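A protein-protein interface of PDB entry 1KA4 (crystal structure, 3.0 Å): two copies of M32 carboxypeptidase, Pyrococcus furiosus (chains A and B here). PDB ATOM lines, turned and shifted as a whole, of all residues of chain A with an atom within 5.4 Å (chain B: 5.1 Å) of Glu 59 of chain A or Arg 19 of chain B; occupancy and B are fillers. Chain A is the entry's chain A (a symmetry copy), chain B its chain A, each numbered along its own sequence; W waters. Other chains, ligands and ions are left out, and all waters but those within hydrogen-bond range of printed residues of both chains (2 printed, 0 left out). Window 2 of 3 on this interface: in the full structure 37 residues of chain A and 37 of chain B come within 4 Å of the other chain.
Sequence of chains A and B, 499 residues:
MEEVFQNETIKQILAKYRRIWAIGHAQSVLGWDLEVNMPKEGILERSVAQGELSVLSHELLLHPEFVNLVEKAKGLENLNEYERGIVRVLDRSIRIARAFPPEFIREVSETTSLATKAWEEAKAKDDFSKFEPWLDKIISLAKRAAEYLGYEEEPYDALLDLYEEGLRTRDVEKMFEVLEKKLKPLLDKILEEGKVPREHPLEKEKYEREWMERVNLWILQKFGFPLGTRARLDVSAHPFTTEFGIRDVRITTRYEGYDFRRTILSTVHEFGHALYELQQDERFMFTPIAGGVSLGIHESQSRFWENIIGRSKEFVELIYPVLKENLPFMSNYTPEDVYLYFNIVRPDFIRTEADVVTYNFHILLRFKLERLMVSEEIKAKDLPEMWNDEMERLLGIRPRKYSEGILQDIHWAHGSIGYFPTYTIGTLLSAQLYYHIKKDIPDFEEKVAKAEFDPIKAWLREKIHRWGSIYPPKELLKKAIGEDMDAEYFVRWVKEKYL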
ATOM      1  N   GLU A  52      -5.530  30.547  -5.456  1.00  0.00           N
ATOM      2  CA  GLU A  52      -6.178  29.310  -5.030  1.00  0.00           C
ATOM      3  C   GLU A  52      -5.161  28.259  -4.620  1.00  0.00           C
ATOM      4  O   GLU A  52      -5.424  27.477  -3.705  1.00  0.00           O
ATOM      5  CB  GLU A  52      -7.055  28.724  -6.138  1.00  0.00           C
ATOM      6  CG  GLU A  52      -8.385  29.425  -6.434  1.00  0.00           C
ATOM      7  CD  GLU A  52      -9.346  29.503  -5.246  1.00  0.00           C
ATOM      8  OE1 GLU A  52      -9.340  28.616  -4.362  1.00  0.00           O
ATOM      9  OE2 GLU A  52     -10.139  30.458  -5.201  1.00  0.00           O
ATOM     10  N   SER A  54      -2.007  28.862  -3.481  1.00  0.00           N
ATOM     11  CA  SER A  54      -1.314  29.288  -2.274  1.00  0.00           C
ATOM     12  C   SER A  54      -2.122  28.894  -1.067  1.00  0.00           C
ATOM     13  O   SER A  54      -1.566  28.477  -0.062  1.00  0.00           O
ATOM     14  CB  SER A  54      -1.087  30.791  -2.272  1.00  0.00           C
ATOM     15  OG  SER A  54      -0.090  31.114  -3.216  1.00  0.00           O
ATOM     16  N   VAL A  55      -3.436  29.023  -1.149  1.00  0.00           N
ATOM     17  CA  VAL A  55      -4.248  28.631  -0.015  1.00  0.00           C
ATOM     18  C   VAL A  55      -4.204  27.100   0.108  1.00  0.00           C
ATOM     19  O   VAL A  55      -4.081  26.558   1.200  1.00  0.00           O
ATOM     20  CB  VAL A  55      -5.696  29.137  -0.175  1.00  0.00           C
ATOM     21  CG1 VAL A  55      -6.596  28.537   0.890  1.00  0.00           C
ATOM     22  CG2 VAL A  55      -5.711  30.638  -0.069  1.00  0.00           C
ATOM     23  N   LEU A  56      -4.266  26.407  -1.028  1.00  0.00           N
ATOM     24  CA  LEU A  56      -4.228  24.951  -1.035  1.00  0.00           C
ATOM     25  C   LEU A  56      -2.922  24.484  -0.402  1.00  0.00           C
ATOM     26  O   LEU A  56      -2.905  23.636   0.507  1.00  0.00           O
ATOM     27  CB  LEU A  56      -4.299  24.425  -2.465  1.00  0.00           C
ATOM     28  CG  LEU A  56      -5.042  23.099  -2.677  1.00  0.00           C
ATOM     29  CD1 LEU A  56      -4.716  22.588  -4.081  1.00  0.00           C
ATOM     30  CD2 LEU A  56      -4.654  22.075  -1.616  1.00  0.00           C
ATOM     31  N   SER A  57      -1.822  25.034  -0.907  1.00  0.00           N
ATOM     32  CA  SER A  57      -0.508  24.694  -0.398  1.00  0.00           C
ATOM     33  C   SER A  57      -0.497  24.835   1.127  1.00  0.00           C
ATOM     34  O   SER A  57      -0.234  23.872   1.844  1.00  0.00           O
ATOM     35  CB  SER A  57       0.535  25.608  -1.020  1.00  0.00           C
ATOM     36  OG  SER A  57       1.814  25.045  -0.840  1.00  0.00           O
ATOM     37  N   HIS A  58      -0.812  26.037   1.607  1.00  0.00           N
ATOM     38  CA  HIS A  58      -0.861  26.351   3.032  1.00  0.00           C
ATOM     39  C   HIS A  58      -1.714  25.331   3.792  1.00  0.00           C
ATOM     40  O   HIS A  58      -1.343  24.870   4.875  1.00  0.00           O
ATOM     41  CB  HIS A  58      -1.436  27.762   3.224  1.00  0.00           C
ATOM     42  CG  HIS A  58      -1.544  28.197   4.658  1.00  0.00           C
ATOM     43  ND1 HIS A  58      -0.440  28.447   5.449  1.00  0.00           N
ATOM     44  CD2 HIS A  58      -2.628  28.440   5.435  1.00  0.00           C
ATOM     45  CE1 HIS A  58      -0.839  28.821   6.651  1.00  0.00           C
ATOM     46  NE2 HIS A  58      -2.161  28.824   6.670  1.00  0.00           N
ATOM     47  N   GLU A  59      -2.857  24.978   3.216  1.00  0.00           N
ATOM     48  CA  GLU A  59      -3.767  24.032   3.844  1.00  0.00           C
ATOM     49  C   GLU A  59      -3.143  22.656   4.017  1.00  0.00           C
ATOM     50  O   GLU A  59      -3.322  22.010   5.052  1.00  0.00           O
ATOM     51  CB  GLU A  59      -5.039  23.923   3.011  1.00  0.00           C
ATOM     52  CG  GLU A  59      -6.049  22.947   3.550  1.00  0.00           C
ATOM     53  CD  GLU A  59      -7.370  23.017   2.811  1.00  0.00           C
ATOM     54  OE1 GLU A  59      -7.930  24.139   2.736  1.00  0.00           O
ATOM     55  OE2 GLU A  59      -7.842  21.953   2.324  1.00  0.00           O
ATOM     56  N   LEU A  60      -2.408  22.215   2.994  1.00  0.00           N
ATOM     57  CA  LEU A  60      -1.746  20.907   3.001  1.00  0.00           C
ATOM     58  C   LEU A  60      -0.600  20.868   4.006  1.00  0.00           C
ATOM     59  O   LEU A  60      -0.403  19.875   4.707  1.00  0.00           O
ATOM     60  CB  LEU A  60      -1.212  20.576   1.602  1.00  0.00           C
ATOM     61  CG  LEU A  60      -2.215  20.274   0.483  1.00  0.00           C
ATOM     62  CD1 LEU A  60      -1.460  20.067  -0.825  1.00  0.00           C
ATOM     63  CD2 LEU A  60      -3.027  19.033   0.823  1.00  0.00           C
ATOM     64  N   LEU A  61       0.161  21.953   4.077  1.00  0.00           N
ATOM     65  CA  LEU A  61       1.277  22.013   4.999  1.00  0.00           C
ATOM     66  C   LEU A  61       0.790  21.927   6.446  1.00  0.00           C
ATOM     67  O   LEU A  61       1.458  21.356   7.304  1.00  0.00           O
ATOM     68  CB  LEU A  61       2.062  23.304   4.800  1.00  0.00           C
ATOM     69  CG  LEU A  61       3.317  23.484   5.671  1.00  0.00           C
ATOM     70  CD1 LEU A  61       4.403  22.493   5.234  1.00  0.00           C
ATOM     71  CD2 LEU A  61       3.822  24.924   5.544  1.00  0.00           C
ATOM     72  N   LEU A  62      -0.379  22.481   6.718  1.00  0.00           N
ATOM     73  CA  LEU A  62      -0.870  22.464   8.081  1.00  0.00           C
ATOM     74  C   LEU A  62      -1.894  21.379   8.377  1.00  0.00           C
ATOM     75  O   LEU A  62      -2.546  21.403   9.423  1.00  0.00           O
ATOM     76  CB  LEU A  62      -1.442  23.838   8.444  1.00  0.00           C
ATOM     77  CG  LEU A  62      -0.468  24.898   8.945  1.00  0.00           C
ATOM     78  CD1 LEU A  62       0.734  24.983   8.059  1.00  0.00           C
ATOM     79  CD2 LEU A  62      -1.191  26.205   9.008  1.00  0.00           C
ATOM     80  N   HIS A  63      -2.040  20.419   7.473  1.00  0.00           N
ATOM     81  CA  HIS A  63      -3.004  19.358   7.725  1.00  0.00           C
ATOM     82  C   HIS A  63      -2.563  18.586   8.971  1.00  0.00           C
ATOM     83  O   HIS A  63      -1.377  18.286   9.146  1.00  0.00           O
ATOM     84  CB  HIS A  63      -3.107  18.425   6.521  1.00  0.00           C
ATOM     85  CG  HIS A  63      -4.296  17.522   6.573  1.00  0.00           C
ATOM     86  ND1 HIS A  63      -4.421  16.509   7.504  1.00  0.00           N
ATOM     87  CD2 HIS A  63      -5.435  17.506   5.838  1.00  0.00           C
ATOM     88  CE1 HIS A  63      -5.587  15.908   7.337  1.00  0.00           C
ATOM     89  NE2 HIS A  63      -6.222  16.495   6.334  1.00  0.00           N
ATOM     90  N   ALA B  15     -17.347  27.971  -5.785  1.00  0.00           N
ATOM     91  CA  ALA B  15     -16.247  28.407  -4.916  1.00  0.00           C
ATOM     92  C   ALA B  15     -15.266  27.270  -4.726  1.00  0.00           C
ATOM     93  O   ALA B  15     -14.059  27.436  -4.838  1.00  0.00           O
ATOM     94  CB  ALA B  15     -16.773  28.849  -3.572  1.00  0.00           C
ATOM     95  N   LYS B  16     -15.789  26.100  -4.415  1.00  0.00           N
ATOM     96  CA  LYS B  16     -14.928  24.955  -4.271  1.00  0.00           C
ATOM     97  C   LYS B  16     -14.316  24.643  -5.647  1.00  0.00           C
ATOM     98  O   LYS B  16     -13.143  24.326  -5.760  1.00  0.00           O
ATOM     99  CB  LYS B  16     -15.735  23.768  -3.766  1.00  0.00           C
ATOM    100  CG  LYS B  16     -16.061  23.850  -2.302  1.00  0.00           C
ATOM    101  CD  LYS B  16     -16.880  22.645  -1.889  1.00  0.00           C
ATOM    102  CE  LYS B  16     -16.968  22.510  -0.368  1.00  0.00           C
ATOM    103  NZ  LYS B  16     -15.638  22.253   0.231  1.00  0.00           N
ATOM    104  N   TYR B  17     -15.116  24.760  -6.699  1.00  0.00           N
ATOM    105  CA  TYR B  17     -14.635  24.466  -8.031  1.00  0.00           C
ATOM    106  C   TYR B  17     -13.428  25.291  -8.436  1.00  0.00           C
ATOM    107  O   TYR B  17     -12.609  24.835  -9.240  1.00  0.00           O
ATOM    108  CB  TYR B  17     -15.730  24.674  -9.060  1.00  0.00           C
ATOM    109  CG  TYR B  17     -15.331  24.148 -10.407  1.00  0.00           C
ATOM    110  CD1 TYR B  17     -15.184  22.782 -10.630  1.00  0.00           C
ATOM    111  CD2 TYR B  17     -15.087  25.013 -11.467  1.00  0.00           C
ATOM    112  CE1 TYR B  17     -14.817  22.291 -11.873  1.00  0.00           C
ATOM    113  CE2 TYR B  17     -14.716  24.535 -12.714  1.00  0.00           C
ATOM    114  CZ  TYR B  17     -14.591  23.177 -12.908  1.00  0.00           C
ATOM    115  OH  TYR B  17     -14.295  22.710 -14.158  1.00  0.00           O
ATOM    116  N   ARG B  18     -13.299  26.500  -7.902  1.00  0.00           N
ATOM    117  CA  ARG B  18     -12.156  27.337  -8.263  1.00  0.00           C
ATOM    118  C   ARG B  18     -10.839  26.618  -8.033  1.00  0.00           C
ATOM    119  O   ARG B  18      -9.915  26.723  -8.836  1.00  0.00           O
ATOM    120  CB  ARG B  18     -12.188  28.646  -7.484  1.00  0.00           C
ATOM    121  CG  ARG B  18     -13.122  29.648  -8.078  1.00  0.00           C
ATOM    122  CD  ARG B  18     -12.691  31.052  -7.758  1.00  0.00           C
ATOM    123  NE  ARG B  18     -13.502  32.035  -8.469  1.00  0.00           N
ATOM    124  CZ  ARG B  18     -13.250  33.337  -8.475  1.00  0.00           C
ATOM    125  NH1 ARG B  18     -12.205  33.802  -7.807  1.00  0.00           N
ATOM    126  NH2 ARG B  18     -14.037  34.171  -9.147  1.00  0.00           N
ATOM    127  N   ARG B  19     -10.754  25.890  -6.929  1.00  0.00           N
ATOM    128  CA  ARG B  19      -9.557  25.132  -6.627  1.00  0.00           C
ATOM    129  C   ARG B  19      -9.288  24.116  -7.709  1.00  0.00           C
ATOM    130  O   ARG B  19      -8.166  23.978  -8.189  1.00  0.00           O
ATOM    131  CB  ARG B  19      -9.710  24.380  -5.322  1.00  0.00           C
ATOM    132  CG  ARG B  19      -9.143  25.093  -4.181  1.00  0.00           C
ATOM    133  CD  ARG B  19      -9.140  24.223  -2.962  1.00  0.00           C
ATOM    134  NE  ARG B  19      -8.653  24.996  -1.834  1.00  0.00           N
ATOM    135  CZ  ARG B  19      -8.507  24.518  -0.616  1.00  0.00           C
ATOM    136  NH1 ARG B  19      -8.820  23.265  -0.380  1.00  0.00           N
ATOM    137  NH2 ARG B  19      -8.038  25.299   0.343  1.00  0.00           N
ATOM    138  N   ILE B  20     -10.326  23.375  -8.068  1.00  0.00           N
ATOM    139  CA  ILE B  20     -10.209  22.357  -9.082  1.00  0.00           C
ATOM    140  C   ILE B  20      -9.796  23.038 -10.385  1.00  0.00           C
ATOM    141  O   ILE B  20      -8.916  22.549 -11.111  1.00  0.00           O
ATOM    142  CB  ILE B  20     -11.533  21.590  -9.245  1.00  0.00           C
ATOM    143  CG1 ILE B  20     -11.815  20.805  -7.957  1.00  0.00           C
ATOM    144  CG2 ILE B  20     -11.453  20.654 -10.432  1.00  0.00           C
ATOM    145  CD1 ILE B  20     -13.150  20.062  -7.967  1.00  0.00           C
ATOM    146  N   TRP B  21     -10.421  24.188 -10.654  1.00  0.00           N
ATOM    147  CA  TRP B  21     -10.150  24.977 -11.845  1.00  0.00           C
ATOM    148  C   TRP B  21      -8.686  25.455 -11.872  1.00  0.00           C
ATOM    149  O   TRP B  21      -8.039  25.487 -12.932  1.00  0.00           O
ATOM    150  CB  TRP B  21     -11.093  26.191 -11.913  1.00  0.00           C
ATOM    151  CG  TRP B  21     -10.761  27.076 -13.072  1.00  0.00           C
ATOM    152  CD1 TRP B  21     -11.151  26.905 -14.363  1.00  0.00           C
ATOM    153  CD2 TRP B  21      -9.809  28.147 -13.079  1.00  0.00           C
ATOM    154  NE1 TRP B  21     -10.495  27.790 -15.185  1.00  0.00           N
ATOM    155  CE2 TRP B  21      -9.664  28.569 -14.423  1.00  0.00           C
ATOM    156  CE3 TRP B  21      -9.059  28.789 -12.080  1.00  0.00           C
ATOM    157  CZ2 TRP B  21      -8.789  29.606 -14.802  1.00  0.00           C
ATOM    158  CZ3 TRP B  21      -8.186  29.822 -12.454  1.00  0.00           C
ATOM    159  CH2 TRP B  21      -8.066  30.218 -13.807  1.00  0.00           C
ATOM    160  N   ALA B  22      -8.180  25.836 -10.698  1.00  0.00           N
ATOM    161  CA  ALA B  22      -6.814  26.312 -10.546  1.00  0.00           C
ATOM    162  C   ALA B  22      -5.786  25.220 -10.872  1.00  0.00           C
ATOM    163  O   ALA B  22      -4.815  25.461 -11.591  1.00  0.00           O
ATOM    164  CB  ALA B  22      -6.618  26.814  -9.150  1.00  0.00           C
ATOM    165  N   ILE B  23      -5.988  24.022 -10.333  1.00  0.00           N
ATOM    166  CA  ILE B  23      -5.081  22.915 -10.628  1.00  0.00           C
ATOM    167  C   ILE B  23      -5.070  22.700 -12.157  1.00  0.00           C
ATOM    168  O   ILE B  23      -4.003  22.525 -12.733  1.00  0.00           O
ATOM    169  CB  ILE B  23      -5.534  21.617  -9.896  1.00  0.00           C
ATOM    170  CG1 ILE B  23      -5.288  21.756  -8.399  1.00  0.00           C
ATOM    171  CG2 ILE B  23      -4.768  20.404 -10.406  1.00  0.00           C
ATOM    172  CD1 ILE B  23      -5.762  20.547  -7.598  1.00  0.00           C
ATOM    173  N   LEU B  60     -10.171  16.033  -5.065  1.00  0.00           N
ATOM    174  CA  LEU B  60     -11.016  17.197  -4.785  1.00  0.00           C
ATOM    175  C   LEU B  60     -12.387  17.060  -5.437  1.00  0.00           C
ATOM    176  O   LEU B  60     -13.411  17.406  -4.847  1.00  0.00           O
ATOM    177  CB  LEU B  60     -10.337  18.478  -5.283  1.00  0.00           C
ATOM    178  CG  LEU B  60      -9.082  18.977  -4.558  1.00  0.00           C
ATOM    179  CD1 LEU B  60      -8.537  20.202  -5.282  1.00  0.00           C
ATOM    180  CD2 LEU B  60      -9.411  19.325  -3.113  1.00  0.00           C
HETATM  181  O   HOH W   1     -10.394  33.185  -5.980  1.00  0.00           O
HETATM  182  O   HOH W   2      -7.710  27.295  -2.969  1.00  0.00           O
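The side-chain carboxylate (OE1) of Glu 59 of chain A lies within salt-bridge range of the guanidinium group (NH2) of Arg 19 of chain B (2.7 Å).
Among the printed residues, pairs that only touch across the chains: Glu 52 of chain A with Arg 18 of chain B, Glu 52 of chain A with Arg 19 of chain B, Glu 52 of chain A with Ala 22 of chain B and Val 55 of chain A with Arg 19 of chain B.
Printed residues of chain B within 4 Å of Glu 52 of chain A: Arg 18, Arg 19 and Ala 22.
Of the printed residues of chain B, Val 55 of chain A touches Arg 19 (3.6 Å).
His 63 of chain A touches none of the printed residues of chain B.
Of the printed residues of chain A, Arg 18 of chain B touches Glu 52 (3.6 Å).
Arg 19 of chain B touches just these residues of chain A: Glu 52 (3.5 Å), Val 55 (3.6 Å) and Glu 59 (2.7 Å).
Of the printed residues of chain A, Ala 22 of chain B touches Glu 52.
The nearest printed residue of chain B that does not touch Glu 59 of chain A is Leu 60 of chain B (6.2 Å).
The nearest printed residue of chain A that does not touch Arg 18 of chain B is Leu 56 of chain A (8.2 Å).
Of the 11 printed residues of chain A, 3 touch a printed residue of chain B.
Printed residues of chain A that touch a printed residue of chain B: Glu 52, Val 55 and Glu 59.
Hydrophobic or aromatic side chains of chain A that line the printed part of chain B: Val 55.
Printed residues of chain B that touch a printed residue of chain A: Arg 18, Arg 19 and Ala 22.
Among the printed residues, Asp or Glu carboxylates within 4 Å of a Lys or Arg side-chain nitrogen of the other chain: Glu 59 of chain A with Arg 19 of chain B.
Position printed for both chains: 60.
Of the 5 pairs that touch across the chains among the printed residues, none has its exchanged pair printed and touching as well.
Water W2 bridges O of Glu 52 of chain A and NE of Arg 19 of chain B.
Water W1 lies within hydrogen-bond range of NH1 of Arg 18 of chain B and OE2 of Glu 52 of chain A.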
